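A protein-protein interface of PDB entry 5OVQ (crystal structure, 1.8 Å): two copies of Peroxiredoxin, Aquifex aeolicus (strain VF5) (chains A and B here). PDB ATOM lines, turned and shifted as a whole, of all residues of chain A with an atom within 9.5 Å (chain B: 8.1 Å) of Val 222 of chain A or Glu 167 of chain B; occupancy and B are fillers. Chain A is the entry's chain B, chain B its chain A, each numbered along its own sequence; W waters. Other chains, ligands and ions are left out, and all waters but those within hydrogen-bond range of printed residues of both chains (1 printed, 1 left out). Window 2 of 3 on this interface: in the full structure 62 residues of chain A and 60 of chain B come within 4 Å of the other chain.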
ATOM      1  N   THR A 146     -15.932 -13.285   7.990  1.00  0.00           N
ATOM      2  CA  THR A 146     -16.282 -14.480   8.750  1.00  0.00           C
ATOM      3  C   THR A 146     -15.842 -15.782   8.098  1.00  0.00           C
ATOM      4  O   THR A 146     -15.742 -16.798   8.803  1.00  0.00           O
ATOM      5  CB  THR A 146     -17.798 -14.587   8.938  1.00  0.00           C
ATOM      6  OG1 THR A 146     -18.444 -14.476   7.655  1.00  0.00           O
ATOM      7  CG2 THR A 146     -18.312 -13.501   9.854  1.00  0.00           C
ATOM      8  N   GLU A 186     -13.669 -34.561   9.901  1.00  0.00           N
ATOM      9  CA  GLU A 186     -14.122 -34.002  11.165  1.00  0.00           C
ATOM     10  C   GLU A 186     -13.355 -32.736  11.517  1.00  0.00           C
ATOM     11  O   GLU A 186     -13.915 -31.800  12.105  1.00  0.00           O
ATOM     12  CB  GLU A 186     -13.968 -35.052  12.272  1.00  0.00           C
ATOM     13  CG  GLU A 186     -14.542 -34.645  13.611  1.00  0.00           C
ATOM     14  CD  GLU A 186     -16.045 -34.450  13.588  1.00  0.00           C
ATOM     15  OE1 GLU A 186     -16.712 -35.010  12.691  1.00  0.00           O
ATOM     16  OE2 GLU A 186     -16.566 -33.739  14.473  1.00  0.00           O
ATOM     17  N   THR A 189     -14.751 -29.540  10.335  1.00  0.00           N
ATOM     18  CA  THR A 189     -16.004 -29.065  10.909  1.00  0.00           C
ATOM     19  C   THR A 189     -15.798 -28.127  12.088  1.00  0.00           C
ATOM     20  O   THR A 189     -16.772 -27.539  12.566  1.00  0.00           O
ATOM     21  CB  THR A 189     -16.873 -30.237  11.371  1.00  0.00           C
ATOM     22  OG1 THR A 189     -16.288 -30.855  12.533  1.00  0.00           O
ATOM     23  CG2 THR A 189     -17.014 -31.271  10.247  1.00  0.00           C
ATOM     24  N   LYS A 190     -14.577 -28.005  12.601  1.00  0.00           N
ATOM     25  CA  LYS A 190     -14.352 -27.116  13.733  1.00  0.00           C
ATOM     26  C   LYS A 190     -14.508 -25.669  13.303  1.00  0.00           C
ATOM     27  O   LYS A 190     -14.022 -25.273  12.244  1.00  0.00           O
ATOM     28  CB  LYS A 190     -12.962 -27.314  14.327  1.00  0.00           C
ATOM     29  CG  LYS A 190     -12.787 -28.687  14.940  1.00  0.00           C
ATOM     30  CD  LYS A 190     -11.394 -28.854  15.496  1.00  0.00           C
ATOM     31  CE  LYS A 190     -11.217 -30.259  16.055  1.00  0.00           C
ATOM     32  NZ  LYS A 190      -9.838 -30.490  16.556  1.00  0.00           N
ATOM     33  N   VAL A 191     -15.207 -24.890  14.119  1.00  0.00           N
ATOM     34  CA  VAL A 191     -15.384 -23.473  13.859  1.00  0.00           C
ATOM     35  C   VAL A 191     -14.362 -22.689  14.668  1.00  0.00           C
ATOM     36  O   VAL A 191     -13.664 -23.224  15.528  1.00  0.00           O
ATOM     37  CB  VAL A 191     -16.820 -22.996  14.160  1.00  0.00           C
ATOM     38  CG1 VAL A 191     -17.826 -23.715  13.245  1.00  0.00           C
ATOM     39  CG2 VAL A 191     -17.146 -23.173  15.629  1.00  0.00           C
ATOM     40  N   ILE A 192     -14.275 -21.396  14.384  1.00  0.00           N
ATOM     41  CA  ILE A 192     -13.257 -20.517  14.936  1.00  0.00           C
ATOM     42  C   ILE A 192     -13.930 -19.519  15.862  1.00  0.00           C
ATOM     43  O   ILE A 192     -14.948 -18.913  15.503  1.00  0.00           O
ATOM     44  CB  ILE A 192     -12.487 -19.808  13.814  1.00  0.00           C
ATOM     45  CG1 ILE A 192     -11.432 -20.757  13.246  1.00  0.00           C
ATOM     46  CG2 ILE A 192     -11.873 -18.498  14.332  1.00  0.00           C
ATOM     47  CD1 ILE A 192     -10.826 -20.300  11.938  1.00  0.00           C
ATOM     48  N   VAL A 193     -13.372 -19.363  17.055  1.00  0.00           N
ATOM     49  CA  VAL A 193     -13.828 -18.321  17.974  1.00  0.00           C
ATOM     50  C   VAL A 193     -13.290 -16.979  17.484  1.00  0.00           C
ATOM     51  O   VAL A 193     -12.084 -16.876  17.191  1.00  0.00           O
ATOM     52  CB  VAL A 193     -13.358 -18.611  19.396  1.00  0.00           C
ATOM     53  CG1 VAL A 193     -13.938 -17.582  20.359  1.00  0.00           C
ATOM     54  CG2 VAL A 193     -13.745 -20.046  19.803  1.00  0.00           C
ATOM     55  N   PRO A 194     -14.134 -15.964  17.336  1.00  0.00           N
ATOM     56  CA  PRO A 194     -13.648 -14.655  16.870  1.00  0.00           C
ATOM     57  C   PRO A 194     -12.507 -14.182  17.748  1.00  0.00           C
ATOM     58  O   PRO A 194     -12.566 -14.330  18.979  1.00  0.00           O
ATOM     59  CB  PRO A 194     -14.883 -13.751  17.007  1.00  0.00           C
ATOM     60  CG  PRO A 194     -16.042 -14.697  16.818  1.00  0.00           C
ATOM     61  CD  PRO A 194     -15.595 -15.970  17.542  1.00  0.00           C
ATOM     62  N   TYR A 210     -10.676 -23.720  25.298  1.00  0.00           N
ATOM     63  CA  TYR A 210     -10.678 -24.085  23.892  1.00  0.00           C
ATOM     64  C   TYR A 210      -9.362 -24.737  23.482  1.00  0.00           C
ATOM     65  O   TYR A 210      -8.357 -24.689  24.191  1.00  0.00           O
ATOM     66  CB  TYR A 210     -10.879 -22.858  23.007  1.00  0.00           C
ATOM     67  CG  TYR A 210     -12.142 -22.088  23.250  1.00  0.00           C
ATOM     68  CD1 TYR A 210     -13.384 -22.648  22.987  1.00  0.00           C
ATOM     69  CD2 TYR A 210     -12.094 -20.781  23.709  1.00  0.00           C
ATOM     70  CE1 TYR A 210     -14.546 -21.933  23.202  1.00  0.00           C
ATOM     71  CE2 TYR A 210     -13.245 -20.063  23.931  1.00  0.00           C
ATOM     72  CZ  TYR A 210     -14.468 -20.636  23.669  1.00  0.00           C
ATOM     73  OH  TYR A 210     -15.617 -19.906  23.883  1.00  0.00           O
ATOM     74  N   LYS A 219     -10.336 -23.010  18.389  1.00  0.00           N
ATOM     75  CA  LYS A 219     -11.360 -23.763  17.674  1.00  0.00           C
ATOM     76  C   LYS A 219     -12.282 -24.484  18.650  1.00  0.00           C
ATOM     77  O   LYS A 219     -11.907 -24.790  19.787  1.00  0.00           O
ATOM     78  CB  LYS A 219     -10.726 -24.784  16.719  1.00  0.00           C
ATOM     79  CG  LYS A 219      -9.943 -24.161  15.570  1.00  0.00           C
ATOM     80  CD  LYS A 219      -9.109 -25.194  14.800  1.00  0.00           C
ATOM     81  CE  LYS A 219      -8.339 -24.502  13.676  1.00  0.00           C
ATOM     82  NZ  LYS A 219      -7.324 -25.362  13.013  1.00  0.00           N
ATOM     83  N   LYS A 220     -13.500 -24.761  18.188  1.00  0.00           N
ATOM     84  CA  LYS A 220     -14.444 -25.591  18.922  1.00  0.00           C
ATOM     85  C   LYS A 220     -15.388 -26.231  17.915  1.00  0.00           C
ATOM     86  O   LYS A 220     -15.371 -25.902  16.729  1.00  0.00           O
ATOM     87  CB  LYS A 220     -15.259 -24.789  19.937  1.00  0.00           C
ATOM     88  CG  LYS A 220     -16.141 -23.724  19.294  1.00  0.00           C
ATOM     89  CD  LYS A 220     -17.043 -23.084  20.336  1.00  0.00           C
ATOM     90  CE  LYS A 220     -18.110 -22.205  19.699  1.00  0.00           C
ATOM     91  NZ  LYS A 220     -19.003 -21.584  20.722  1.00  0.00           N
ATOM     92  N   LYS A 221     -16.261 -27.102  18.400  1.00  0.00           N
ATOM     93  CA  LYS A 221     -17.307 -27.643  17.547  1.00  0.00           C
ATOM     94  C   LYS A 221     -18.658 -27.064  17.942  1.00  0.00           C
ATOM     95  O   LYS A 221     -18.868 -26.621  19.074  1.00  0.00           O
ATOM     96  CB  LYS A 221     -17.334 -29.172  17.602  1.00  0.00           C
ATOM     97  CG  LYS A 221     -16.124 -29.789  16.941  1.00  0.00           C
ATOM     98  CD  LYS A 221     -16.206 -31.291  16.923  1.00  0.00           C
ATOM     99  CE  LYS A 221     -14.946 -31.870  16.332  1.00  0.00           C
ATOM    100  NZ  LYS A 221     -15.027 -33.342  16.355  1.00  0.00           N
ATOM    101  N   VAL A 222     -19.580 -27.084  16.990  1.00  0.00           N
ATOM    102  CA  VAL A 222     -20.925 -26.586  17.223  1.00  0.00           C
ATOM    103  C   VAL A 222     -21.856 -27.757  17.512  1.00  0.00           C
ATOM    104  O   VAL A 222     -22.001 -28.667  16.693  1.00  0.00           O
ATOM    105  CB  VAL A 222     -21.430 -25.775  16.016  1.00  0.00           C
ATOM    106  CG1 VAL A 222     -22.915 -25.514  16.143  1.00  0.00           C
ATOM    107  CG2 VAL A 222     -20.658 -24.474  15.892  1.00  0.00           C
ATOM    108  N   ALA A 223     -22.476 -27.719  18.690  1.00  0.00           N
ATOM    109  CA  ALA A 223     -23.331 -28.800  19.184  1.00  0.00           C
ATOM    110  C   ALA A 223     -24.489 -29.127  18.244  1.00  0.00           C
ATOM    111  O   ALA A 223     -25.360 -29.932  18.586  1.00  0.00           O
ATOM    112  CB  ALA A 223     -23.885 -28.441  20.565  1.00  0.00           C
ATOM    113  N   ALA B 160     -21.749 -21.920   5.747  1.00  0.00           N
ATOM    114  CA  ALA B 160     -20.747 -21.206   6.535  1.00  0.00           C
ATOM    115  C   ALA B 160     -21.287 -19.872   7.030  1.00  0.00           C
ATOM    116  O   ALA B 160     -21.105 -19.509   8.201  1.00  0.00           O
ATOM    117  CB  ALA B 160     -19.490 -20.995   5.690  1.00  0.00           C
ATOM    118  N   LEU B 161     -21.996 -19.145   6.158  1.00  0.00           N
ATOM    119  CA  LEU B 161     -22.533 -17.851   6.552  1.00  0.00           C
ATOM    120  C   LEU B 161     -23.651 -18.030   7.567  1.00  0.00           C
ATOM    121  O   LEU B 161     -23.735 -17.288   8.545  1.00  0.00           O
ATOM    122  CB  LEU B 161     -23.027 -17.089   5.312  1.00  0.00           C
ATOM    123  CG  LEU B 161     -21.945 -16.626   4.327  1.00  0.00           C
ATOM    124  CD1 LEU B 161     -22.549 -16.279   2.979  1.00  0.00           C
ATOM    125  CD2 LEU B 161     -21.189 -15.394   4.901  1.00  0.00           C
ATOM    126  N   GLN B 162     -24.510 -19.022   7.366  1.00  0.00           N
ATOM    127  CA  GLN B 162     -25.592 -19.220   8.330  1.00  0.00           C
ATOM    128  C   GLN B 162     -25.054 -19.681   9.678  1.00  0.00           C
ATOM    129  O   GLN B 162     -25.592 -19.303  10.728  1.00  0.00           O
ATOM    130  CB  GLN B 162     -26.608 -20.228   7.790  1.00  0.00           C
ATOM    131  CG  GLN B 162     -27.369 -19.709   6.574  1.00  0.00           C
ATOM    132  CD  GLN B 162     -28.429 -20.664   6.069  1.00  0.00           C
ATOM    133  OE1 GLN B 162     -28.393 -21.860   6.350  1.00  0.00           O
ATOM    134  NE2 GLN B 162     -29.392 -20.132   5.313  1.00  0.00           N
ATOM    135  N   THR B 163     -24.024 -20.529   9.667  1.00  0.00           N
ATOM    136  CA  THR B 163     -23.411 -20.975  10.918  1.00  0.00           C
ATOM    137  C   THR B 163     -22.743 -19.816  11.644  1.00  0.00           C
ATOM    138  O   THR B 163     -22.882 -19.675  12.865  1.00  0.00           O
ATOM    139  CB  THR B 163     -22.389 -22.079  10.632  1.00  0.00           C
ATOM    140  OG1 THR B 163     -23.058 -23.253  10.149  1.00  0.00           O
ATOM    141  CG2 THR B 163     -21.584 -22.425  11.886  1.00  0.00           C
ATOM    142  N   ALA B 164     -22.015 -18.981  10.904  1.00  0.00           N
ATOM    143  CA  ALA B 164     -21.400 -17.798  11.505  1.00  0.00           C
ATOM    144  C   ALA B 164     -22.451 -16.934  12.193  1.00  0.00           C
ATOM    145  O   ALA B 164     -22.284 -16.536  13.353  1.00  0.00           O
ATOM    146  CB  ALA B 164     -20.642 -17.011  10.442  1.00  0.00           C
ATOM    147  N   ASP B 165     -23.565 -16.666  11.504  1.00  0.00           N
ATOM    148  CA  ASP B 165     -24.639 -15.878  12.105  1.00  0.00           C
ATOM    149  C   ASP B 165     -25.267 -16.598  13.288  1.00  0.00           C
ATOM    150  O   ASP B 165     -25.520 -15.989  14.332  1.00  0.00           O
ATOM    151  CB  ASP B 165     -25.725 -15.567  11.077  1.00  0.00           C
ATOM    152  CG  ASP B 165     -25.284 -14.578  10.039  1.00  0.00           C
ATOM    153  OD1 ASP B 165     -24.127 -14.093  10.100  1.00  0.00           O
ATOM    154  OD2 ASP B 165     -26.119 -14.284   9.161  1.00  0.00           O
ATOM    155  N   ARG B 166     -25.561 -17.894  13.137  1.00  0.00           N
ATOM    156  CA  ARG B 166     -26.277 -18.602  14.195  1.00  0.00           C
ATOM    157  C   ARG B 166     -25.416 -18.767  15.441  1.00  0.00           C
ATOM    158  O   ARG B 166     -25.909 -18.625  16.566  1.00  0.00           O
ATOM    159  CB  ARG B 166     -26.743 -19.975  13.697  1.00  0.00           C
ATOM    160  CG  ARG B 166     -27.551 -20.766  14.726  1.00  0.00           C
ATOM    161  CD  ARG B 166     -27.869 -22.191  14.238  1.00  0.00           C
ATOM    162  NE  ARG B 166     -26.653 -22.976  14.034  1.00  0.00           N
ATOM    163  CZ  ARG B 166     -26.157 -23.297  12.843  1.00  0.00           C
ATOM    164  NH1 ARG B 166     -26.780 -22.912  11.735  1.00  0.00           N
ATOM    165  NH2 ARG B 166     -25.041 -24.008  12.759  1.00  0.00           N
ATOM    166  N   GLU B 167     -24.136 -19.080  15.266  1.00  0.00           N
ATOM    167  CA  GLU B 167     -23.290 -19.460  16.390  1.00  0.00           C
ATOM    168  C   GLU B 167     -22.347 -18.359  16.858  1.00  0.00           C
ATOM    169  O   GLU B 167     -21.690 -18.532  17.892  1.00  0.00           O
ATOM    170  CB  GLU B 167     -22.490 -20.719  16.041  1.00  0.00           C
ATOM    171  CG  GLU B 167     -23.366 -21.892  15.599  1.00  0.00           C
ATOM    172  CD  GLU B 167     -24.186 -22.476  16.744  1.00  0.00           C
ATOM    173  OE1 GLU B 167     -23.809 -22.283  17.920  1.00  0.00           O
ATOM    174  OE2 GLU B 167     -25.202 -23.147  16.469  1.00  0.00           O
ATOM    175  N   GLY B 168     -22.260 -17.246  16.137  1.00  0.00           N
ATOM    176  CA  GLY B 168     -21.316 -16.196  16.480  1.00  0.00           C
ATOM    177  C   GLY B 168     -19.876 -16.633  16.320  1.00  0.00           C
ATOM    178  O   GLY B 168     -19.033 -16.342  17.184  1.00  0.00           O
ATOM    179  N   VAL B 169     -19.570 -17.317  15.227  1.00  0.00           N
ATOM    180  CA  VAL B 169     -18.256 -17.888  15.009  1.00  0.00           C
ATOM    181  C   VAL B 169     -17.788 -17.490  13.631  1.00  0.00           C
ATOM    182  O   VAL B 169     -18.542 -16.943  12.823  1.00  0.00           O
ATOM    183  CB  VAL B 169     -18.272 -19.426  15.142  1.00  0.00           C
ATOM    184  CG1 VAL B 169     -18.716 -19.822  16.540  1.00  0.00           C
ATOM    185  CG2 VAL B 169     -19.194 -20.033  14.076  1.00  0.00           C
ATOM    186  N   ALA B 170     -16.530 -17.789  13.363  1.00  0.00           N
ATOM    187  CA  ALA B 170     -16.004 -17.731  12.015  1.00  0.00           C
ATOM    188  C   ALA B 170     -15.757 -19.151  11.525  1.00  0.00           C
ATOM    189  O   ALA B 170     -15.674 -20.094  12.320  1.00  0.00           O
ATOM    190  CB  ALA B 170     -14.717 -16.901  11.968  1.00  0.00           C
ATOM    191  N   THR B 171     -15.638 -19.302  10.198  1.00  0.00           N
ATOM    192  CA  THR B 171     -15.371 -20.636   9.708  1.00  0.00           C
ATOM    193  C   THR B 171     -14.022 -20.665   9.011  1.00  0.00           C
ATOM    194  O   THR B 171     -13.700 -19.767   8.228  1.00  0.00           O
ATOM    195  CB  THR B 171     -16.461 -21.162   8.727  1.00  0.00           C
ATOM    196  OG1 THR B 171     -16.585 -20.281   7.603  1.00  0.00           O
ATOM    197  CG2 THR B 171     -17.808 -21.252   9.438  1.00  0.00           C
ATOM    198  N   TRP B 175     -14.103 -25.211   5.537  1.00  0.00           N
ATOM    199  CA  TRP B 175     -15.042 -25.656   6.566  1.00  0.00           C
ATOM    200  C   TRP B 175     -16.281 -26.309   5.967  1.00  0.00           C
ATOM    201  O   TRP B 175     -16.820 -25.836   4.960  1.00  0.00           O
ATOM    202  CB  TRP B 175     -15.499 -24.488   7.427  1.00  0.00           C
ATOM    203  CG  TRP B 175     -16.511 -24.859   8.490  1.00  0.00           C
ATOM    204  CD1 TRP B 175     -16.240 -25.350   9.748  1.00  0.00           C
ATOM    205  CD2 TRP B 175     -17.936 -24.750   8.404  1.00  0.00           C
ATOM    206  NE1 TRP B 175     -17.413 -25.544  10.442  1.00  0.00           N
ATOM    207  CE2 TRP B 175     -18.466 -25.186   9.637  1.00  0.00           C
ATOM    208  CE3 TRP B 175     -18.818 -24.328   7.400  1.00  0.00           C
ATOM    209  CZ2 TRP B 175     -19.834 -25.204   9.892  1.00  0.00           C
ATOM    210  CZ3 TRP B 175     -20.177 -24.350   7.658  1.00  0.00           C
ATOM    211  CH2 TRP B 175     -20.672 -24.781   8.891  1.00  0.00           C
ATOM    212  N   PRO B 177     -20.128 -28.243   7.636  1.00  0.00           N
ATOM    213  CA  PRO B 177     -20.861 -28.468   8.892  1.00  0.00           C
ATOM    214  C   PRO B 177     -20.732 -29.886   9.419  1.00  0.00           C
ATOM    215  O   PRO B 177     -20.847 -30.095  10.635  1.00  0.00           O
ATOM    216  CB  PRO B 177     -22.312 -28.141   8.519  1.00  0.00           C
ATOM    217  CG  PRO B 177     -22.375 -28.296   7.042  1.00  0.00           C
ATOM    218  CD  PRO B 177     -21.029 -27.902   6.522  1.00  0.00           C
HETATM  219  O   HOH W   1     -18.679 -18.186   8.016  1.00  0.00           O
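O of Glu 186 of chain A is in hydrogen-bond range of OG1 of Thr 189 of chain A, 2.6 Å away. N of Val 191 of chain A is in hydrogen-bond range of O of Lys 220 of chain A (2.8 Å). The backbone carbonyl oxygen (O) of Ala 164 of chain B lies within hydrogen-bond range of the backbone NH (N) of Val 169 of chain B, 3.4 Å away. NE of Arg 166 of chain B lies within salt-bridge range of OE2 of Glu 167 of chain B, at 2.8 Å.
N of Thr 171 of chain B is in hydrogen-bond range of O of Thr 146 of chain A (2.9 Å). The backbone carbonyl oxygen (O) of Ala 170 of chain B lies within hydrogen-bond range of the backbone NH (N) of Ile 192 of chain A (2.8 Å). The backbone carbonyl oxygen of Thr 189 of chain A sits at hydrogen-bond distance from the indole nitrogen of Trp 175 of chain B (3.0 Å).
No position is printed for both chains.
Among the printed residues, pairs that only touch across the chains: Thr 146 of chain A with Leu 161 of chain B, Thr 146 of chain A with Ala 170 of chain B, Lys 190 of chain A with Trp 175 of chain B, Val 191 of chain A with Val 169 of chain B, Val 191 of chain A with Ala 170 of chain B, Val 191 of chain A with Trp 175 of chain B, Ile 192 of chain A with Val 169 of chain B, Pro 194 of chain A with Gly 168 of chain B and Val 222 of chain A with Glu 167 of chain B.
Water W1 lies within hydrogen-bond range of O of Ala 160 of chain B (2.8 Å), OG1 of Thr 171 of chain B (3.0 Å) and O of Thr 146 of chain A (3.3 Å).
Printed residues of chain B within 4 Å of Lys 190 of chain A: Trp 175. Of the printed residues of chain B, Ile 192 of chain A touches Val 169 and Ala 170. Val 222 of chain A touches one residue of chain B. Printed residues of chain A within 4 Å of Leu 161 of chain B: Thr 146 (3.995 Å). Glu 167 of chain B touches just one residue of chain A: Val 222. Of the printed residues of chain A, Gly 168 of chain B touches Pro 194. Of the printed residues of chain A, Thr 171 of chain B touches Thr 146. The nearest residue of chain B that does not touch Val 222 of chain A is Arg 166 of chain B (4.3 Å). The nearest residue of chain A that does not touch Glu 167 of chain B is Lys 220 of chain A (5.0 Å). The nearest printed residue of chain A that does not touch Thr 171 of chain B is Ile 192 of chain A (4.3 Å).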
